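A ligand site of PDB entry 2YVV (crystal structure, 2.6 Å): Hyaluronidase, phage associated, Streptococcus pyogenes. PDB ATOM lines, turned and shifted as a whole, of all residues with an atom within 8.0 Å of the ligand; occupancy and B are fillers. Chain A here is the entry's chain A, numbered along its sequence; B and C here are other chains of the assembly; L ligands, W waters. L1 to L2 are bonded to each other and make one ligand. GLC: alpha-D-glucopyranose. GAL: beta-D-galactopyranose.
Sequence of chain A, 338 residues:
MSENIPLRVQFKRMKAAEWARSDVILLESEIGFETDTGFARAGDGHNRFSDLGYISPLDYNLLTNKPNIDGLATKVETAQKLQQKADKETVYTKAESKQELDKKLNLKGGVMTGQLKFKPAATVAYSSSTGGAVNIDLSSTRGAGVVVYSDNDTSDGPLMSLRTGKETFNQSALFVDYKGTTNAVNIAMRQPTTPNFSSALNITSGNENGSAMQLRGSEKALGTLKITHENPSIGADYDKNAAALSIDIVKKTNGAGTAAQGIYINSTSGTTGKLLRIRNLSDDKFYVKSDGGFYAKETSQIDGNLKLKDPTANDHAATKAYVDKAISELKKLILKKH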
ATOM      1  N   ARG A 163      22.081  -8.789 -30.471  1.00  0.00           N
ATOM      2  CA  ARG A 163      22.482 -10.208 -30.535  1.00  0.00           C
ATOM      3  C   ARG A 163      23.590 -10.533 -29.520  1.00  0.00           C
ATOM      4  O   ARG A 163      24.575  -9.799 -29.388  1.00  0.00           O
ATOM      5  CB  ARG A 163      22.929 -10.583 -31.960  1.00  0.00           C
ATOM      6  CG  ARG A 163      23.071 -12.126 -32.255  1.00  0.00           C
ATOM      7  CD  ARG A 163      23.822 -12.468 -33.581  1.00  0.00           C
ATOM      8  NE  ARG A 163      25.112 -11.741 -33.665  1.00  0.00           N
ATOM      9  CZ  ARG A 163      26.269 -12.155 -33.138  1.00  0.00           C
ATOM     10  NH1 ARG A 163      26.319 -13.306 -32.473  1.00  0.00           N
ATOM     11  NH2 ARG A 163      27.377 -11.432 -33.243  1.00  0.00           N
ATOM     12  N   THR A 164      23.408 -11.622 -28.791  1.00  0.00           N
ATOM     13  CA  THR A 164      24.508 -12.141 -27.990  1.00  0.00           C
ATOM     14  C   THR A 164      24.835 -13.577 -28.402  1.00  0.00           C
ATOM     15  O   THR A 164      23.936 -14.421 -28.558  1.00  0.00           O
ATOM     16  CB  THR A 164      24.188 -12.099 -26.517  1.00  0.00           C
ATOM     17  OG1 THR A 164      22.947 -12.794 -26.282  1.00  0.00           O
ATOM     18  CG2 THR A 164      24.114 -10.645 -26.082  1.00  0.00           C
ATOM     19  N   GLY A 165      26.120 -13.865 -28.585  1.00  0.00           N
ATOM     20  CA  GLY A 165      26.529 -15.125 -29.193  1.00  0.00           C
ATOM     21  C   GLY A 165      26.953 -16.249 -28.236  1.00  0.00           C
ATOM     22  O   GLY A 165      27.048 -17.383 -28.653  1.00  0.00           O
ATOM     23  N   LYS A 166      27.186 -15.967 -26.967  1.00  0.00           N
ATOM     24  CA  LYS A 166      27.730 -17.024 -26.076  1.00  0.00           C
ATOM     25  C   LYS A 166      26.798 -17.382 -24.942  1.00  0.00           C
ATOM     26  O   LYS A 166      26.304 -16.523 -24.251  1.00  0.00           O
ATOM     27  CB  LYS A 166      29.085 -16.604 -25.470  1.00  0.00           C
ATOM     28  CG  LYS A 166      30.213 -16.356 -26.454  1.00  0.00           C
ATOM     29  CD  LYS A 166      31.122 -17.568 -26.584  1.00  0.00           C
ATOM     30  CE  LYS A 166      30.977 -18.261 -27.928  1.00  0.00           C
ATOM     31  NZ  LYS A 166      31.752 -17.753 -29.093  1.00  0.00           N
ATOM     32  N   GLU A 167      26.648 -18.671 -24.687  1.00  0.00           N
ATOM     33  CA  GLU A 167      25.720 -19.124 -23.669  1.00  0.00           C
ATOM     34  C   GLU A 167      26.006 -18.735 -22.232  1.00  0.00           C
ATOM     35  O   GLU A 167      25.143 -18.833 -21.356  1.00  0.00           O
ATOM     36  CB  GLU A 167      25.499 -20.618 -23.830  1.00  0.00           C
ATOM     37  CG  GLU A 167      24.177 -20.900 -24.597  1.00  0.00           C
ATOM     38  CD  GLU A 167      22.922 -20.329 -23.846  1.00  0.00           C
ATOM     39  OE1 GLU A 167      22.728 -20.685 -22.656  1.00  0.00           O
ATOM     40  OE2 GLU A 167      22.148 -19.526 -24.443  1.00  0.00           O
ATOM     41  N   TYR B 149      25.984  -6.088 -30.893  1.00  0.00           N
ATOM     42  CA  TYR B 149      26.083  -7.491 -30.550  1.00  0.00           C
ATOM     43  C   TYR B 149      27.328  -7.755 -29.799  1.00  0.00           C
ATOM     44  O   TYR B 149      28.279  -6.957 -29.804  1.00  0.00           O
ATOM     45  CB  TYR B 149      26.094  -8.353 -31.807  1.00  0.00           C
ATOM     46  CG  TYR B 149      27.151  -7.878 -32.746  1.00  0.00           C
ATOM     47  CD1 TYR B 149      26.941  -6.730 -33.525  1.00  0.00           C
ATOM     48  CD2 TYR B 149      28.393  -8.515 -32.816  1.00  0.00           C
ATOM     49  CE1 TYR B 149      27.937  -6.244 -34.380  1.00  0.00           C
ATOM     50  CE2 TYR B 149      29.396  -8.048 -33.682  1.00  0.00           C
ATOM     51  CZ  TYR B 149      29.155  -6.910 -34.459  1.00  0.00           C
ATOM     52  OH  TYR B 149      30.119  -6.411 -35.304  1.00  0.00           O
ATOM     53  N   SER B 150      27.362  -8.902 -29.160  1.00  0.00           N
ATOM     54  CA  SER B 150      28.547  -9.288 -28.475  1.00  0.00           C
ATOM     55  C   SER B 150      28.701 -10.780 -28.579  1.00  0.00           C
ATOM     56  O   SER B 150      27.713 -11.531 -28.438  1.00  0.00           O
ATOM     57  CB  SER B 150      28.446  -8.904 -27.015  1.00  0.00           C
ATOM     58  OG  SER B 150      29.544  -9.477 -26.302  1.00  0.00           O
ATOM     59  N   ASP B 151      29.938 -11.203 -28.853  1.00  0.00           N
ATOM     60  CA  ASP B 151      30.298 -12.606 -28.754  1.00  0.00           C
ATOM     61  C   ASP B 151      31.251 -12.884 -27.594  1.00  0.00           C
ATOM     62  O   ASP B 151      31.971 -13.863 -27.584  1.00  0.00           O
ATOM     63  CB  ASP B 151      30.831 -13.090 -30.086  1.00  0.00           C
ATOM     64  CG  ASP B 151      29.720 -13.133 -31.128  1.00  0.00           C
ATOM     65  OD1 ASP B 151      28.804 -13.984 -30.966  1.00  0.00           O
ATOM     66  OD2 ASP B 151      29.723 -12.284 -32.078  1.00  0.00           O
ATOM     67  N   ASN B 152      31.219 -12.011 -26.590  1.00  0.00           N
ATOM     68  CA  ASN B 152      32.056 -12.140 -25.411  1.00  0.00           C
ATOM     69  C   ASN B 152      31.454 -13.145 -24.446  1.00  0.00           C
ATOM     70  O   ASN B 152      30.254 -13.413 -24.486  1.00  0.00           O
ATOM     71  CB  ASN B 152      32.203 -10.798 -24.748  1.00  0.00           C
ATOM     72  CG  ASN B 152      33.519 -10.666 -24.008  1.00  0.00           C
ATOM     73  OD1 ASN B 152      34.257 -11.642 -23.898  1.00  0.00           O
ATOM     74  ND2 ASN B 152      33.817  -9.460 -23.497  1.00  0.00           N
ATOM     75  N   ASP B 153      32.263 -13.727 -23.595  1.00  0.00           N
ATOM     76  CA  ASP B 153      31.749 -14.802 -22.780  1.00  0.00           C
ATOM     77  C   ASP B 153      30.916 -14.238 -21.664  1.00  0.00           C
ATOM     78  O   ASP B 153      29.922 -14.836 -21.265  1.00  0.00           O
ATOM     79  CB  ASP B 153      32.888 -15.604 -22.175  1.00  0.00           C
ATOM     80  CG  ASP B 153      33.856 -16.068 -23.216  1.00  0.00           C
ATOM     81  OD1 ASP B 153      33.462 -16.940 -24.045  1.00  0.00           O
ATOM     82  OD2 ASP B 153      34.990 -15.533 -23.226  1.00  0.00           O
ATOM     83  N   ARG B 190      17.120 -18.501 -27.878  1.00  0.00           N
ATOM     84  CA  ARG B 190      17.631 -19.722 -28.518  1.00  0.00           C
ATOM     85  C   ARG B 190      17.827 -20.875 -27.550  1.00  0.00           C
ATOM     86  O   ARG B 190      18.331 -20.676 -26.463  1.00  0.00           O
ATOM     87  CB  ARG B 190      19.005 -19.385 -29.153  1.00  0.00           C
ATOM     88  CG  ARG B 190      19.000 -18.114 -30.068  1.00  0.00           C
ATOM     89  CD  ARG B 190      18.393 -18.532 -31.407  1.00  0.00           C
ATOM     90  NE  ARG B 190      18.217 -17.440 -32.373  1.00  0.00           N
ATOM     91  CZ  ARG B 190      17.180 -17.365 -33.213  1.00  0.00           C
ATOM     92  NH1 ARG B 190      16.227 -18.292 -33.165  1.00  0.00           N
ATOM     93  NH2 ARG B 190      17.082 -16.363 -34.075  1.00  0.00           N
ATOM     94  N   SER C 129      25.710  -9.629 -38.186  1.00  0.00           N
ATOM     95  CA  SER C 129      26.638  -8.941 -37.263  1.00  0.00           C
ATOM     96  C   SER C 129      27.750  -8.106 -37.967  1.00  0.00           C
ATOM     97  O   SER C 129      28.872  -7.988 -37.456  1.00  0.00           O
ATOM     98  CB  SER C 129      27.255  -9.934 -36.258  1.00  0.00           C
ATOM     99  OG  SER C 129      28.144 -10.853 -36.866  1.00  0.00           O
ATOM    100  N   THR C 130      27.416  -7.525 -39.119  1.00  0.00           N
ATOM    101  CA  THR C 130      28.362  -6.668 -39.852  1.00  0.00           C
ATOM    102  C   THR C 130      27.634  -5.576 -40.682  1.00  0.00           C
ATOM    103  O   THR C 130      28.263  -4.829 -41.466  1.00  0.00           O
ATOM    104  CB  THR C 130      29.401  -7.520 -40.686  1.00  0.00           C
ATOM    105  OG1 THR C 130      30.262  -6.660 -41.453  1.00  0.00           O
ATOM    106  CG2 THR C 130      28.704  -8.499 -41.614  1.00  0.00           C
ATOM    107  N   ASP C 137      30.246  -3.615 -31.765  1.00  0.00           N
ATOM    108  CA  ASP C 137      30.731  -4.959 -31.506  1.00  0.00           C
ATOM    109  C   ASP C 137      31.396  -4.920 -30.141  1.00  0.00           C
ATOM    110  O   ASP C 137      32.475  -4.317 -29.990  1.00  0.00           O
ATOM    111  CB  ASP C 137      31.757  -5.354 -32.568  1.00  0.00           C
ATOM    112  CG  ASP C 137      32.368  -6.740 -32.337  1.00  0.00           C
ATOM    113  OD1 ASP C 137      32.103  -7.402 -31.300  1.00  0.00           O
ATOM    114  OD2 ASP C 137      33.119  -7.188 -33.216  1.00  0.00           O
ATOM    115  N   SER C 139      32.310  -7.674 -28.496  1.00  0.00           N
ATOM    116  CA  SER C 139      32.973  -8.968 -28.320  1.00  0.00           C
ATOM    117  C   SER C 139      34.261  -8.998 -27.502  1.00  0.00           C
ATOM    118  O   SER C 139      34.573 -10.017 -26.919  1.00  0.00           O
ATOM    119  CB  SER C 139      33.206  -9.664 -29.661  1.00  0.00           C
ATOM    120  OG  SER C 139      31.975  -9.842 -30.327  1.00  0.00           O
ATOM    121  N   ASP C 177      18.029 -11.370 -30.453  1.00  0.00           N
ATOM    122  CA  ASP C 177      18.498 -12.739 -30.657  1.00  0.00           C
ATOM    123  C   ASP C 177      19.445 -13.022 -29.494  1.00  0.00           C
ATOM    124  O   ASP C 177      20.583 -12.537 -29.465  1.00  0.00           O
ATOM    125  CB  ASP C 177      19.230 -12.798 -31.998  1.00  0.00           C
ATOM    126  CG  ASP C 177      19.694 -14.212 -32.398  1.00  0.00           C
ATOM    127  OD1 ASP C 177      19.490 -15.173 -31.626  1.00  0.00           O
ATOM    128  OD2 ASP C 177      20.264 -14.359 -33.516  1.00  0.00           O
ATOM    129  N   TYR C 178      18.996 -13.772 -28.506  1.00  0.00           N
ATOM    130  CA  TYR C 178      19.740 -13.765 -27.250  1.00  0.00           C
ATOM    131  C   TYR C 178      20.224 -15.124 -26.849  1.00  0.00           C
ATOM    132  O   TYR C 178      19.448 -16.057 -26.832  1.00  0.00           O
ATOM    133  CB  TYR C 178      18.879 -13.274 -26.113  1.00  0.00           C
ATOM    134  CG  TYR C 178      19.574 -13.247 -24.788  1.00  0.00           C
ATOM    135  CD1 TYR C 178      20.431 -12.193 -24.445  1.00  0.00           C
ATOM    136  CD2 TYR C 178      19.349 -14.265 -23.840  1.00  0.00           C
ATOM    137  CE1 TYR C 178      21.055 -12.149 -23.184  1.00  0.00           C
ATOM    138  CE2 TYR C 178      19.969 -14.224 -22.566  1.00  0.00           C
ATOM    139  CZ  TYR C 178      20.816 -13.152 -22.243  1.00  0.00           C
ATOM    140  OH  TYR C 178      21.442 -13.067 -20.999  1.00  0.00           O
ATOM    141  N   LYS C 179      21.494 -15.196 -26.469  1.00  0.00           N
ATOM    142  CA  LYS C 179      22.052 -16.362 -25.748  1.00  0.00           C
ATOM    143  C   LYS C 179      22.657 -15.827 -24.481  1.00  0.00           C
ATOM    144  O   LYS C 179      23.268 -14.786 -24.531  1.00  0.00           O
ATOM    145  CB  LYS C 179      23.119 -17.084 -26.570  1.00  0.00           C
ATOM    146  CG  LYS C 179      22.508 -17.741 -27.763  1.00  0.00           C
ATOM    147  CD  LYS C 179      23.383 -18.790 -28.410  1.00  0.00           C
ATOM    148  CE  LYS C 179      22.886 -19.033 -29.858  1.00  0.00           C
ATOM    149  NZ  LYS C 179      23.650 -20.135 -30.512  1.00  0.00           N
HETATM  150  C1  GLC L   1      26.924 -18.486 -33.209  1.00  0.00           C
HETATM  151  C2  GLC L   1      27.390 -18.424 -31.775  1.00  0.00           C
HETATM  152  C3  GLC L   1      28.709 -17.506 -31.717  1.00  0.00           C
HETATM  153  C4  GLC L   1      29.786 -18.206 -32.567  1.00  0.00           C
HETATM  154  C5  GLC L   1      29.263 -18.392 -34.036  1.00  0.00           C
HETATM  155  C6  GLC L   1      30.312 -19.158 -34.909  1.00  0.00           C
HETATM  156  O1  GLC L   1      26.658 -17.109 -33.605  1.00  0.00           O
HETATM  157  O2  GLC L   1      26.322 -17.857 -31.004  1.00  0.00           O
HETATM  158  O3  GLC L   1      29.202 -17.391 -30.366  1.00  0.00           O
HETATM  159  O4  GLC L   1      31.181 -17.704 -32.730  1.00  0.00           O
HETATM  160  O5  GLC L   1      27.960 -19.106 -34.046  1.00  0.00           O
HETATM  161  O6  GLC L   1      29.806 -19.346 -36.234  1.00  0.00           O
HETATM  162  C1  GAL L   2      31.753 -16.331 -32.560  1.00  0.00           C
HETATM  163  C2  GAL L   2      33.280 -16.680 -32.756  1.00  0.00           C
HETATM  164  C3  GAL L   2      34.178 -15.460 -32.680  1.00  0.00           C
HETATM  165  C4  GAL L   2      33.636 -14.476 -33.797  1.00  0.00           C
HETATM  166  C5  GAL L   2      32.111 -14.088 -33.618  1.00  0.00           C
HETATM  167  C6  GAL L   2      31.708 -13.166 -34.851  1.00  0.00           C
HETATM  168  O2  GAL L   2      33.700 -17.604 -31.744  1.00  0.00           O
HETATM  169  O3  GAL L   2      35.611 -15.897 -32.904  1.00  0.00           O
HETATM  170  O4  GAL L   2      33.879 -15.031 -35.121  1.00  0.00           O
HETATM  171  O5  GAL L   2      31.387 -15.396 -33.668  1.00  0.00           O
HETATM  172  O6  GAL L   2      31.318 -11.816 -34.511  1.00  0.00           O
HETATM  173  O   HOH W   1      24.356 -16.718 -34.650  1.00  0.00           O
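O of Gly 165 is in hydrogen-bond range of O2 of GLC L1 (2.5 Å). O3 of GLC L1 sits at hydrogen-bond distance from NZ of Lys 166, at 2.9 Å. O6 of GAL L2 lies within hydrogen-bond range of OD2 of Asp 151 of chain B (2.9 Å).
N of Gly 165 lies within hydrogen-bond range of O of Ser 150 of chain B (2.8 Å). The side-chain carboxylate (OD2) of Asp 151 of chain B is in salt-bridge range of the guanidinium group (NH2) of Arg 163 (2.8 Å). The backbone NH (N) of Asp 151 of chain B sits at hydrogen-bond distance from the side-chain hydroxyl (OG) of Ser 139 of chain C (2.9 Å). The backbone carbonyl oxygen (O) of Lys 179 of chain C sits at hydrogen-bond distance from the side-chain hydroxyl (OG1) of Thr 164 (2.7 Å). N of Ser 150 of chain B sits at hydrogen-bond distance from O of Arg 163 (2.9 Å).
Residues that only touch the ligand: Lys 179 of chain C (3.5 Å) and Arg 163 (3.98 Å). Of the 18 residues printed, 5 come within 4 Å of the ligand.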
